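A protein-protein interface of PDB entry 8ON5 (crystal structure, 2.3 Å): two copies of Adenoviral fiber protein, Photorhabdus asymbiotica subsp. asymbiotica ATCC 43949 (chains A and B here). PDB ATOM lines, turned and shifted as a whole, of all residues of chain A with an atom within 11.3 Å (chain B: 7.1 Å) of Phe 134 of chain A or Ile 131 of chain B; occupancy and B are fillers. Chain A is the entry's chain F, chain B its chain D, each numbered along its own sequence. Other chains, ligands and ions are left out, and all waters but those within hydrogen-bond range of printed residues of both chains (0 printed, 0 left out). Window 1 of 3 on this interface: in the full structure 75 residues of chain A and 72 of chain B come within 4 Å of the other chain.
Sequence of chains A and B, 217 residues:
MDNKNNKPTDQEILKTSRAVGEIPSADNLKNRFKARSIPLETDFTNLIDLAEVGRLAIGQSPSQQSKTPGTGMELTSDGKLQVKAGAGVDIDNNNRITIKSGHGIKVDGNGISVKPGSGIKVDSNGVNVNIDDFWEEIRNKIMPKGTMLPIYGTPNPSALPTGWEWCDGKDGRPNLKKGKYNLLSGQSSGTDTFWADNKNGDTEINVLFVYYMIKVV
Printed residues of chain B within 4 Å of Ser 118 of chain A: Asn 128 and Val 129.
Printed residues of chain B within 4 Å of Gly 119 of chain A: Val 129.
Printed residues of chain B within 4 Å of Phe 134 of chain A: Ile 131.
Printed residues of chain B within 4 Å of Lys 141 of chain A: Ile 131 (3.6 Å) and Trp 135 (3.6 Å).
Printed residues of chain B within 4 Å of Ile 142 of chain A: Trp 135 (3.9 Å).
No residue of chain A comes within 4 Å of Gly 119 of chain B.
Of the printed residues of chain A, Val 129 of chain B touches Ser 118 (2.8 Å), Gly 119 (3.3 Å) and Ile 120 (3.9 Å).
No residue of chain A comes within 4 Å of Asn 130 of chain B.
Of the printed residues of chain A, Ile 131 of chain B touches Phe 134 (3.4 Å), Glu 137 (3.6 Å), Ile 138 (3.7 Å) and Lys 141 (3.6 Å).
No residue of chain A comes within 4 Å of Asp 132 of chain B.
No residue of chain A comes within 4 Å of Asp 133 of chain B.
No residue of chain A comes within 4 Å of Phe 134 of chain B.
The nearest printed residue of chain B that does not touch Phe 134 of chain A is Val 129 of chain B (4.02 Å).
The nearest residue of chain A that does not touch Ile 131 of chain B is Trp 135 of chain A (6.2 Å).
The backbone NH (N) of Asn 130 of chain A is in hydrogen-bond range of the backbone carbonyl oxygen (O) of Gly 119 of chain A (2.7 Å).
The backbone NH (N) of Gly 119 of chain A sits at hydrogen-bond distance from the side-chain carboxylate (OD2) of Asp 133 of chain A (2.7 Å).
Gly 119 of chain A touches Val 129 of chain B, but with the chains exchanged Val 129 of chain A does not touch Gly 119 of chain B (7.1 Å).
Phe 134 of chain A touches Ile 131 of chain B, but with the chains exchanged Ile 131 of chain A does not touch Phe 134 of chain B (7.8 Å).
Ile 138 of chain A touches Ile 131 of chain B, but with the chains exchanged Ile 131 of chain A does not touch Ile 138 of chain B (7.5 Å).
Ile 138 of chain A touches Trp 135 of chain B, but with the chains exchanged Trp 135 of chain A does not touch Ile 138 of chain B (7.9 Å).
Positions printed for both chains: 119, 120, 128, 129, 130, 131, 132, 133, 134, 135, 136 and 138.
Among the printed residues, merely in contact across the chains: Gly 117 of chain A with Asn 128 of chain B (3.3 Å), Gly 119 of chain A with Val 129 of chain B (3.3 Å), Ile 120 of chain A with Val 129 of chain B (3.9 Å), Phe 134 of chain A with Ile 131 of chain B (3.4 Å), Glu 137 of chain A with Ile 131 of chain B (3.6 Å), Ile 138 of chain A with Ile 131 of chain B (3.7 Å), Ile 138 of chain A with Trp 135 of chain B (3.8 Å), Lys 141 of chain A with Ile 131 of chain B (3.6 Å), Lys 141 of chain A with Trp 135 of chain B (3.6 Å) and Ile 142 of chain A with Trp 135 of chain B (3.9 Å).
The backbone NH (N) of Val 129 of chain B sits at hydrogen-bond distance from the backbone carbonyl oxygen (O) of Ser 118 of chain A (2.8 Å).
OD1 of Asn 128 of chain B sits at hydrogen-bond distance from N of Ser 118 of chain A.
Hydrophobic or aromatic side chains of chain B within 4 Å of the printed part of chain A: Val 129, Ile 131 and Trp 135.
Along chain B the printed residues that touch a printed residue of chain A span positions 128 to 135.
Among the printed residues, 12 pairs touch across the chains.
Among the printed residues, no Asp or Glu carboxylate lies within 4 Å of a Lys or Arg side-chain nitrogen of the other chain.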
ATOM      1  N   GLY A 117     -11.538  27.700  21.822  1.00  0.00           N
ATOM      2  CA  GLY A 117     -11.935  28.118  20.482  1.00  0.00           C
ATOM      3  C   GLY A 117     -12.736  27.046  19.740  1.00  0.00           C
ATOM      4  O   GLY A 117     -13.408  26.219  20.346  1.00  0.00           O
ATOM      5  N   SER A 118     -12.616  27.009  18.408  1.00  0.00           N
ATOM      6  CA  SER A 118     -13.371  26.016  17.640  1.00  0.00           C
ATOM      7  C   SER A 118     -12.906  24.594  17.950  1.00  0.00           C
ATOM      8  O   SER A 118     -11.734  24.277  17.792  1.00  0.00           O
ATOM      9  CB  SER A 118     -13.272  26.246  16.169  1.00  0.00           C
ATOM     10  OG  SER A 118     -14.202  25.404  15.513  1.00  0.00           O
ATOM     11  N   GLY A 119     -13.835  23.748  18.392  1.00  0.00           N
ATOM     12  CA  GLY A 119     -13.560  22.334  18.557  1.00  0.00           C
ATOM     13  C   GLY A 119     -12.979  21.981  19.922  1.00  0.00           C
ATOM     14  O   GLY A 119     -12.537  20.837  20.127  1.00  0.00           O
ATOM     15  N   ILE A 120     -13.016  22.960  20.844  1.00  0.00           N
ATOM     16  CA  ILE A 120     -12.399  22.818  22.152  1.00  0.00           C
ATOM     17  C   ILE A 120     -13.400  23.196  23.239  1.00  0.00           C
ATOM     18  O   ILE A 120     -14.116  24.181  23.121  1.00  0.00           O
ATOM     19  CB  ILE A 120     -11.127  23.677  22.233  1.00  0.00           C
ATOM     20  CG1 ILE A 120     -10.038  23.119  21.325  1.00  0.00           C
ATOM     21  CG2 ILE A 120     -10.650  23.772  23.673  1.00  0.00           C
ATOM     22  CD1 ILE A 120      -9.647  21.684  21.662  1.00  0.00           C
ATOM     23  N   LYS A 121     -13.414  22.396  24.298  1.00  0.00           N
ATOM     24  CA  LYS A 121     -14.207  22.656  25.484  1.00  0.00           C
ATOM     25  C   LYS A 121     -13.267  22.496  26.690  1.00  0.00           C
ATOM     26  O   LYS A 121     -12.467  21.554  26.758  1.00  0.00           O
ATOM     27  CB  LYS A 121     -15.456  21.761  25.453  1.00  0.00           C
ATOM     28  CG  LYS A 121     -15.992  21.245  26.785  1.00  0.00           C
ATOM     29  N   VAL A 127      -8.188  20.603  28.897  1.00  0.00           N
ATOM     30  CA  VAL A 127      -8.568  20.985  27.550  1.00  0.00           C
ATOM     31  C   VAL A 127      -9.073  19.730  26.837  1.00  0.00           C
ATOM     32  O   VAL A 127      -8.339  18.753  26.734  1.00  0.00           O
ATOM     33  CB  VAL A 127      -7.393  21.642  26.799  1.00  0.00           C
ATOM     34  CG1 VAL A 127      -7.794  22.078  25.400  1.00  0.00           C
ATOM     35  CG2 VAL A 127      -6.817  22.816  27.578  1.00  0.00           C
ATOM     36  N   ASN A 128     -10.320  19.774  26.354  1.00  0.00           N
ATOM     37  CA  ASN A 128     -10.942  18.626  25.713  1.00  0.00           C
ATOM     38  C   ASN A 128     -11.339  19.009  24.300  1.00  0.00           C
ATOM     39  O   ASN A 128     -11.640  20.180  24.022  1.00  0.00           O
ATOM     40  CB  ASN A 128     -12.223  18.129  26.400  1.00  0.00           C
ATOM     41  CG  ASN A 128     -12.027  17.856  27.874  1.00  0.00           C
ATOM     42  OD1 ASN A 128     -11.600  16.770  28.253  1.00  0.00           O
ATOM     43  ND2 ASN A 128     -12.315  18.840  28.707  1.00  0.00           N
ATOM     44  N   VAL A 129     -11.386  17.980  23.446  1.00  0.00           N
ATOM     45  CA  VAL A 129     -11.819  18.148  22.076  1.00  0.00           C
ATOM     46  C   VAL A 129     -13.335  18.036  22.073  1.00  0.00           C
ATOM     47  O   VAL A 129     -13.866  17.143  22.722  1.00  0.00           O
ATOM     48  CB  VAL A 129     -11.176  17.089  21.171  1.00  0.00           C
ATOM     49  CG1 VAL A 129     -11.846  17.039  19.812  1.00  0.00           C
ATOM     50  CG2 VAL A 129      -9.678  17.296  21.043  1.00  0.00           C
ATOM     51  N   ASN A 130     -14.010  18.942  21.347  1.00  0.00           N
ATOM     52  CA  ASN A 130     -15.438  18.827  21.109  1.00  0.00           C
ATOM     53  C   ASN A 130     -15.708  18.640  19.615  1.00  0.00           C
ATOM     54  O   ASN A 130     -15.522  19.570  18.826  1.00  0.00           O
ATOM     55  CB  ASN A 130     -16.180  20.051  21.645  1.00  0.00           C
ATOM     56  CG  ASN A 130     -17.663  20.033  21.329  1.00  0.00           C
ATOM     57  OD1 ASN A 130     -18.344  19.032  21.558  1.00  0.00           O
ATOM     58  ND2 ASN A 130     -18.162  21.131  20.783  1.00  0.00           N
ATOM     59  N   ILE A 131     -16.204  17.459  19.219  1.00  0.00           N
ATOM     60  CA  ILE A 131     -16.262  17.122  17.793  1.00  0.00           C
ATOM     61  C   ILE A 131     -17.374  17.875  17.054  1.00  0.00           C
ATOM     62  O   ILE A 131     -17.224  18.158  15.868  1.00  0.00           O
ATOM     63  CB  ILE A 131     -16.407  15.608  17.566  1.00  0.00           C
ATOM     64  CG1 ILE A 131     -17.791  15.119  17.997  1.00  0.00           C
ATOM     65  CG2 ILE A 131     -15.268  14.856  18.240  1.00  0.00           C
ATOM     66  CD1 ILE A 131     -18.016  13.632  17.812  1.00  0.00           C
ATOM     67  N   ASP A 132     -18.476  18.204  17.743  1.00  0.00           N
ATOM     68  CA  ASP A 132     -19.617  18.861  17.114  1.00  0.00           C
ATOM     69  C   ASP A 132     -19.185  20.051  16.257  1.00  0.00           C
ATOM     70  O   ASP A 132     -19.868  20.413  15.309  1.00  0.00           O
ATOM     71  CB  ASP A 132     -20.661  19.313  18.132  1.00  0.00           C
ATOM     72  CG  ASP A 132     -21.256  18.196  18.978  1.00  0.00           C
ATOM     73  OD1 ASP A 132     -21.099  16.994  18.619  1.00  0.00           O
ATOM     74  OD2 ASP A 132     -21.860  18.538  20.012  1.00  0.00           O
ATOM     75  N   ASP A 133     -18.038  20.666  16.527  1.00  0.00           N
ATOM     76  CA  ASP A 133     -17.687  21.845  15.746  1.00  0.00           C
ATOM     77  C   ASP A 133     -17.088  21.468  14.397  1.00  0.00           C
ATOM     78  O   ASP A 133     -17.023  22.330  13.530  1.00  0.00           O
ATOM     79  CB  ASP A 133     -16.739  22.797  16.489  1.00  0.00           C
ATOM     80  CG  ASP A 133     -17.306  23.463  17.744  1.00  0.00           C
ATOM     81  OD1 ASP A 133     -18.564  23.531  17.899  1.00  0.00           O
ATOM     82  OD2 ASP A 133     -16.474  23.896  18.586  1.00  0.00           O
ATOM     83  N   PHE A 134     -16.579  20.239  14.212  1.00  0.00           N
ATOM     84  CA  PHE A 134     -15.770  20.005  13.023  1.00  0.00           C
ATOM     85  C   PHE A 134     -16.042  18.644  12.380  1.00  0.00           C
ATOM     86  O   PHE A 134     -15.518  18.392  11.311  1.00  0.00           O
ATOM     87  CB  PHE A 134     -14.279  20.213  13.328  1.00  0.00           C
ATOM     88  CG  PHE A 134     -13.721  19.245  14.338  1.00  0.00           C
ATOM     89  CD1 PHE A 134     -13.258  17.996  13.954  1.00  0.00           C
ATOM     90  CD2 PHE A 134     -13.736  19.537  15.689  1.00  0.00           C
ATOM     91  CE1 PHE A 134     -12.778  17.087  14.886  1.00  0.00           C
ATOM     92  CE2 PHE A 134     -13.259  18.629  16.622  1.00  0.00           C
ATOM     93  CZ  PHE A 134     -12.773  17.407  16.224  1.00  0.00           C
ATOM     94  N   TRP A 135     -16.837  17.760  12.977  1.00  0.00           N
ATOM     95  CA  TRP A 135     -16.961  16.422  12.408  1.00  0.00           C
ATOM     96  C   TRP A 135     -17.556  16.481  11.002  1.00  0.00           C
ATOM     97  O   TRP A 135     -17.131  15.718  10.142  1.00  0.00           O
ATOM     98  CB  TRP A 135     -17.732  15.443  13.310  1.00  0.00           C
ATOM     99  CG  TRP A 135     -19.210  15.644  13.336  1.00  0.00           C
ATOM    100  CD1 TRP A 135     -19.913  16.480  14.148  1.00  0.00           C
ATOM    101  CD2 TRP A 135     -20.176  15.001  12.495  1.00  0.00           C
ATOM    102  NE1 TRP A 135     -21.251  16.382  13.891  1.00  0.00           N
ATOM    103  CE2 TRP A 135     -21.444  15.492  12.876  1.00  0.00           C
ATOM    104  CE3 TRP A 135     -20.096  14.055  11.468  1.00  0.00           C
ATOM    105  CZ2 TRP A 135     -22.617  15.085  12.254  1.00  0.00           C
ATOM    106  CZ3 TRP A 135     -21.261  13.645  10.855  1.00  0.00           C
ATOM    107  CH2 TRP A 135     -22.502  14.154  11.244  1.00  0.00           C
ATOM    108  N   GLU A 136     -18.512  17.392  10.778  1.00  0.00           N
ATOM    109  CA  GLU A 136     -19.154  17.515   9.481  1.00  0.00           C
ATOM    110  C   GLU A 136     -18.129  17.913   8.421  1.00  0.00           C
ATOM    111  O   GLU A 136     -18.224  17.440   7.289  1.00  0.00           O
ATOM    112  CB  GLU A 136     -20.353  18.462   9.519  1.00  0.00           C
ATOM    113  CG  GLU A 136     -21.509  17.912  10.345  1.00  0.00           C
ATOM    114  CD  GLU A 136     -22.728  18.820  10.478  1.00  0.00           C
ATOM    115  OE1 GLU A 136     -22.679  19.954   9.974  1.00  0.00           O
ATOM    116  OE2 GLU A 136     -23.731  18.389  11.089  1.00  0.00           O
ATOM    117  N   GLU A 137     -17.146  18.749   8.759  1.00  0.00           N
ATOM    118  CA  GLU A 137     -16.162  19.113   7.753  1.00  0.00           C
ATOM    119  C   GLU A 137     -15.273  17.903   7.440  1.00  0.00           C
ATOM    120  O   GLU A 137     -14.786  17.773   6.322  1.00  0.00           O
ATOM    121  CB  GLU A 137     -15.358  20.365   8.131  1.00  0.00           C
ATOM    122  CG  GLU A 137     -15.063  21.263   6.918  1.00  0.00           C
ATOM    123  CD  GLU A 137     -13.869  22.211   6.975  1.00  0.00           C
ATOM    124  OE1 GLU A 137     -13.485  22.739   5.901  1.00  0.00           O
ATOM    125  OE2 GLU A 137     -13.316  22.434   8.079  1.00  0.00           O
ATOM    126  N   ILE A 138     -15.069  16.995   8.405  1.00  0.00           N
ATOM    127  CA  ILE A 138     -14.301  15.791   8.127  1.00  0.00           C
ATOM    128  C   ILE A 138     -15.103  14.836   7.226  1.00  0.00           C
ATOM    129  O   ILE A 138     -14.550  14.230   6.312  1.00  0.00           O
ATOM    130  CB  ILE A 138     -13.825  15.132   9.436  1.00  0.00           C
ATOM    131  CG1 ILE A 138     -12.715  15.967  10.088  1.00  0.00           C
ATOM    132  CG2 ILE A 138     -13.381  13.684   9.218  1.00  0.00           C
ATOM    133  CD1 ILE A 138     -12.342  15.483  11.473  1.00  0.00           C
ATOM    134  N   ARG A 139     -16.398  14.697   7.489  1.00  0.00           N
ATOM    135  CA  ARG A 139     -17.286  13.894   6.659  1.00  0.00           C
ATOM    136  C   ARG A 139     -17.142  14.335   5.200  1.00  0.00           C
ATOM    137  O   ARG A 139     -16.821  13.528   4.315  1.00  0.00           O
ATOM    138  CB  ARG A 139     -18.706  14.027   7.223  1.00  0.00           C
ATOM    139  CG  ARG A 139     -19.798  13.312   6.446  1.00  0.00           C
ATOM    140  CD  ARG A 139     -21.173  13.926   6.725  1.00  0.00           C
ATOM    141  NE  ARG A 139     -21.243  15.316   6.281  1.00  0.00           N
ATOM    142  CZ  ARG A 139     -22.167  16.195   6.649  1.00  0.00           C
ATOM    143  NH1 ARG A 139     -23.179  15.829   7.421  1.00  0.00           N
ATOM    144  NH2 ARG A 139     -22.084  17.443   6.212  1.00  0.00           N
ATOM    145  N   ASN A 140     -17.277  15.642   4.970  1.00  0.00           N
ATOM    146  CA  ASN A 140     -17.275  16.162   3.614  1.00  0.00           C
ATOM    147  C   ASN A 140     -15.907  16.027   2.973  1.00  0.00           C
ATOM    148  O   ASN A 140     -15.793  16.087   1.767  1.00  0.00           O
ATOM    149  CB  ASN A 140     -17.657  17.633   3.549  1.00  0.00           C
ATOM    150  CG  ASN A 140     -19.041  17.923   4.093  1.00  0.00           C
ATOM    151  OD1 ASN A 140     -19.860  17.031   4.328  1.00  0.00           O
ATOM    152  ND2 ASN A 140     -19.303  19.195   4.305  1.00  0.00           N
ATOM    153  N   LYS A 141     -14.847  15.867   3.759  1.00  0.00           N
ATOM    154  CA  LYS A 141     -13.548  15.683   3.137  1.00  0.00           C
ATOM    155  C   LYS A 141     -13.410  14.238   2.662  1.00  0.00           C
ATOM    156  O   LYS A 141     -12.561  13.934   1.821  1.00  0.00           O
ATOM    157  CB  LYS A 141     -12.426  16.120   4.084  1.00  0.00           C
ATOM    158  CG  LYS A 141     -12.246  17.625   4.129  1.00  0.00           C
ATOM    159  CD  LYS A 141     -11.143  18.092   5.005  1.00  0.00           C
ATOM    160  CE  LYS A 141     -11.045  19.598   5.035  1.00  0.00           C
ATOM    161  NZ  LYS A 141     -10.606  20.114   3.724  1.00  0.00           N
ATOM    162  N   ILE A 142     -14.249  13.370   3.213  1.00  0.00           N
ATOM    163  CA  ILE A 142     -14.154  11.955   2.959  1.00  0.00           C
ATOM    164  C   ILE A 142     -15.206  11.515   1.946  1.00  0.00           C
ATOM    165  O   ILE A 142     -14.909  10.693   1.100  1.00  0.00           O
ATOM    166  CB  ILE A 142     -14.286  11.178   4.273  1.00  0.00           C
ATOM    167  CG1 ILE A 142     -13.178  11.528   5.258  1.00  0.00           C
ATOM    168  CG2 ILE A 142     -14.277   9.702   3.985  1.00  0.00           C
ATOM    169  CD1 ILE A 142     -13.365  10.861   6.611  1.00  0.00           C
ATOM    170  N   MET A 143     -16.427  12.046   2.023  1.00  0.00           N
ATOM    171  CA  MET A 143     -17.489  11.598   1.140  1.00  0.00           C
ATOM    172  C   MET A 143     -18.224  12.764   0.488  1.00  0.00           C
ATOM    173  O   MET A 143     -18.867  13.548   1.169  1.00  0.00           O
ATOM    174  CB  MET A 143     -18.481  10.754   1.924  1.00  0.00           C
ATOM    175  CG  MET A 143     -17.983   9.343   2.007  1.00  0.00           C
ATOM    176  SD  MET A 143     -19.198   8.326   2.761  1.00  0.00           S
ATOM    177  CE  MET A 143     -19.204   9.030   4.403  1.00  0.00           C
ATOM    178  N   THR A 162     -27.071  12.727   9.754  1.00  0.00           N
ATOM    179  CA  THR A 162     -27.262  14.089   9.287  1.00  0.00           C
ATOM    180  C   THR A 162     -26.570  14.277   7.939  1.00  0.00           C
ATOM    181  O   THR A 162     -25.426  13.842   7.778  1.00  0.00           O
ATOM    182  CB  THR A 162     -26.699  15.104  10.296  1.00  0.00           C
ATOM    183  OG1 THR A 162     -27.482  14.939  11.470  1.00  0.00           O
ATOM    184  CG2 THR A 162     -26.760  16.546   9.832  1.00  0.00           C
ATOM    185  N   LYS A 215     -26.018  11.135   0.089  1.00  0.00           N
ATOM    186  CA  LYS A 215     -25.595  12.299   0.841  1.00  0.00           C
ATOM    187  C   LYS A 215     -26.001  13.535   0.044  1.00  0.00           C
ATOM    188  O   LYS A 215     -25.524  13.700  -1.081  1.00  0.00           O
ATOM    189  CB  LYS A 215     -24.094  12.203   1.120  1.00  0.00           C
ATOM    190  CG  LYS A 215     -23.463  13.407   1.808  1.00  0.00           C
ATOM    191  CD  LYS A 215     -21.985  13.199   2.119  1.00  0.00           C
ATOM    192  CE  LYS A 215     -21.310  14.343   2.851  1.00  0.00           C
ATOM    193  NZ  LYS A 215     -20.635  15.276   1.917  1.00  0.00           N
ATOM    194  N   GLY B 119      -2.614  19.520  15.050  1.00  0.00           N
ATOM    195  CA  GLY B 119      -4.075  19.503  15.063  1.00  0.00           C
ATOM    196  C   GLY B 119      -4.686  20.691  15.797  1.00  0.00           C
ATOM    197  O   GLY B 119      -5.888  20.719  16.059  1.00  0.00           O
ATOM    198  N   ILE B 120      -3.835  21.650  16.164  1.00  0.00           N
ATOM    199  CA  ILE B 120      -4.241  22.756  17.008  1.00  0.00           C
ATOM    200  C   ILE B 120      -3.740  24.039  16.371  1.00  0.00           C
ATOM    201  O   ILE B 120      -2.564  24.146  16.002  1.00  0.00           O
ATOM    202  CB  ILE B 120      -3.680  22.617  18.434  1.00  0.00           C
ATOM    203  CG1 ILE B 120      -4.390  21.515  19.223  1.00  0.00           C
ATOM    204  CG2 ILE B 120      -3.750  23.973  19.162  1.00  0.00           C
ATOM    205  CD1 ILE B 120      -5.883  21.780  19.461  1.00  0.00           C
ATOM    206  N   ASN B 128      -7.823  26.273  19.004  1.00  0.00           N
ATOM    207  CA  ASN B 128      -8.732  25.718  18.003  1.00  0.00           C
ATOM    208  C   ASN B 128      -8.197  24.401  17.445  1.00  0.00           C
ATOM    209  O   ASN B 128      -6.991  24.227  17.271  1.00  0.00           O
ATOM    210  CB  ASN B 128      -8.950  26.645  16.792  1.00  0.00           C
ATOM    211  CG  ASN B 128      -9.346  28.067  17.161  1.00  0.00           C
ATOM    212  OD1 ASN B 128     -10.509  28.356  17.475  1.00  0.00           O
ATOM    213  ND2 ASN B 128      -8.351  28.933  17.173  1.00  0.00           N
ATOM    214  N   VAL B 129      -9.132  23.517  17.100  1.00  0.00           N
ATOM    215  CA  VAL B 129      -8.844  22.333  16.327  1.00  0.00           C
ATOM    216  C   VAL B 129      -8.614  22.736  14.885  1.00  0.00           C
ATOM    217  O   VAL B 129      -9.346  23.529  14.345  1.00  0.00           O
ATOM    218  CB  VAL B 129      -9.958  21.295  16.443  1.00  0.00           C
ATOM    219  CG1 VAL B 129      -9.670  20.092  15.558  1.00  0.00           C
ATOM    220  CG2 VAL B 129     -10.150  20.854  17.884  1.00  0.00           C
ATOM    221  N   ASN B 130      -7.518  22.246  14.328  1.00  0.00           N
ATOM    222  CA  ASN B 130      -7.220  22.316  12.920  1.00  0.00           C
ATOM    223  C   ASN B 130      -7.208  20.884  12.361  1.00  0.00           C
ATOM    224  O   ASN B 130      -6.239  20.157  12.514  1.00  0.00           O
ATOM    225  CB  ASN B 130      -5.893  23.041  12.714  1.00  0.00           C
ATOM    226  CG  ASN B 130      -5.443  22.952  11.274  1.00  0.00           C
ATOM    227  OD1 ASN B 130      -6.163  22.415  10.436  1.00  0.00           O
ATOM    228  ND2 ASN B 130      -4.229  23.375  10.984  1.00  0.00           N
ATOM    229  N   ILE B 131      -8.261  20.500  11.646  1.00  0.00           N
ATOM    230  CA  ILE B 131      -8.393  19.160  11.087  1.00  0.00           C
ATOM    231  C   ILE B 131      -7.372  18.834   9.979  1.00  0.00           C
ATOM    232  O   ILE B 131      -7.145  17.664   9.715  1.00  0.00           O
ATOM    233  CB  ILE B 131      -9.823  18.928  10.581  1.00  0.00           C
ATOM    234  CG1 ILE B 131     -10.221  19.954   9.523  1.00  0.00           C
ATOM    235  CG2 ILE B 131     -10.821  18.864  11.736  1.00  0.00           C
ATOM    236  CD1 ILE B 131     -11.341  19.469   8.624  1.00  0.00           C
ATOM    237  N   ASP B 132      -6.717  19.816   9.349  1.00  0.00           N
ATOM    238  CA  ASP B 132      -5.759  19.506   8.299  1.00  0.00           C
ATOM    239  C   ASP B 132      -4.715  18.489   8.762  1.00  0.00           C
ATOM    240  O   ASP B 132      -4.254  17.643   7.991  1.00  0.00           O
ATOM    241  CB  ASP B 132      -5.042  20.760   7.815  1.00  0.00           C
ATOM    242  CG  ASP B 132      -5.964  21.741   7.107  1.00  0.00           C
ATOM    243  OD1 ASP B 132      -7.190  21.492   7.066  1.00  0.00           O
ATOM    244  OD2 ASP B 132      -5.439  22.760   6.604  1.00  0.00           O
ATOM    245  N   ASP B 133      -4.324  18.567  10.031  1.00  0.00           N
ATOM    246  CA  ASP B 133      -3.223  17.761  10.520  1.00  0.00           C
ATOM    247  C   ASP B 133      -3.653  16.301  10.702  1.00  0.00           C
ATOM    248  O   ASP B 133      -2.779  15.440  10.693  1.00  0.00           O
ATOM    249  CB  ASP B 133      -2.626  18.368  11.798  1.00  0.00           C
ATOM    250  CG  ASP B 133      -1.910  19.699  11.608  1.00  0.00           C
ATOM    251  OD1 ASP B 133      -1.722  20.101  10.440  1.00  0.00           O
ATOM    252  OD2 ASP B 133      -1.543  20.327  12.644  1.00  0.00           O
ATOM    253  N   PHE B 134      -4.957  15.989  10.832  1.00  0.00           N
ATOM    254  CA  PHE B 134      -5.301  14.630  11.206  1.00  0.00           C
ATOM    255  C   PHE B 134      -6.499  13.997  10.488  1.00  0.00           C
ATOM    256  O   PHE B 134      -6.757  12.816  10.741  1.00  0.00           O
ATOM    257  CB  PHE B 134      -5.495  14.565  12.724  1.00  0.00           C
ATOM    258  CG  PHE B 134      -6.628  15.392  13.268  1.00  0.00           C
ATOM    259  CD1 PHE B 134      -7.920  14.903  13.277  1.00  0.00           C
ATOM    260  CD2 PHE B 134      -6.389  16.660  13.789  1.00  0.00           C
ATOM    261  CE1 PHE B 134      -8.956  15.671  13.791  1.00  0.00           C
ATOM    262  CE2 PHE B 134      -7.422  17.424  14.306  1.00  0.00           C
ATOM    263  CZ  PHE B 134      -8.708  16.933  14.293  1.00  0.00           C
ATOM    264  N   TRP B 135      -7.225  14.689   9.591  1.00  0.00           N
ATOM    265  CA  TRP B 135      -8.497  14.121   9.130  1.00  0.00           C
ATOM    266  C   TRP B 135      -8.245  12.877   8.268  1.00  0.00           C
ATOM    267  O   TRP B 135      -9.032  11.929   8.280  1.00  0.00           O
ATOM    268  CB  TRP B 135      -9.368  15.152   8.399  1.00  0.00           C
ATOM    269  CG  TRP B 135      -8.857  15.508   7.038  1.00  0.00           C
ATOM    270  CD1 TRP B 135      -8.031  16.553   6.728  1.00  0.00           C
ATOM    271  CD2 TRP B 135      -9.124  14.832   5.801  1.00  0.00           C
ATOM    272  NE1 TRP B 135      -7.770  16.570   5.391  1.00  0.00           N
ATOM    273  CE2 TRP B 135      -8.419  15.526   4.794  1.00  0.00           C
ATOM    274  CE3 TRP B 135      -9.882  13.719   5.441  1.00  0.00           C
ATOM    275  CZ2 TRP B 135      -8.432  15.134   3.461  1.00  0.00           C
ATOM    276  CZ3 TRP B 135      -9.903  13.331   4.117  1.00  0.00           C
ATOM    277  CH2 TRP B 135      -9.186  14.034   3.143  1.00  0.00           C
ATOM    278  N   GLU B 136      -7.130  12.881   7.546  1.00  0.00           N
ATOM    279  CA  GLU B 136      -6.765  11.773   6.682  1.00  0.00           C
ATOM    280  C   GLU B 136      -6.566  10.485   7.496  1.00  0.00           C
ATOM    281  O   GLU B 136      -7.012   9.396   7.090  1.00  0.00           O
ATOM    282  CB  GLU B 136      -5.527  12.154   5.870  1.00  0.00           C
ATOM    283  CG  GLU B 136      -5.820  13.204   4.817  1.00  0.00           C
ATOM    284  CD  GLU B 136      -4.595  13.745   4.101  1.00  0.00           C
ATOM    285  OE1 GLU B 136      -3.804  14.461   4.747  1.00  0.00           O
ATOM    286  OE2 GLU B 136      -4.433  13.466   2.904  1.00  0.00           O
ATOM    287  N   ILE B 138      -7.973   9.865  10.324  1.00  0.00           N
ATOM    288  CA  ILE B 138      -9.280   9.387  10.748  1.00  0.00           C
ATOM    289  C   ILE B 138      -9.970   8.666   9.584  1.00  0.00           C
ATOM    290  O   ILE B 138     -10.689   7.683   9.776  1.00  0.00           O
ATOM    291  CB  ILE B 138     -10.119  10.562  11.281  1.00  0.00           C
ATOM    292  CG1 ILE B 138      -9.520  11.073  12.598  1.00  0.00           C
ATOM    293  CG2 ILE B 138     -11.587  10.184  11.408  1.00  0.00           C
ATOM    294  CD1 ILE B 138     -10.295  12.204  13.289  1.00  0.00           C
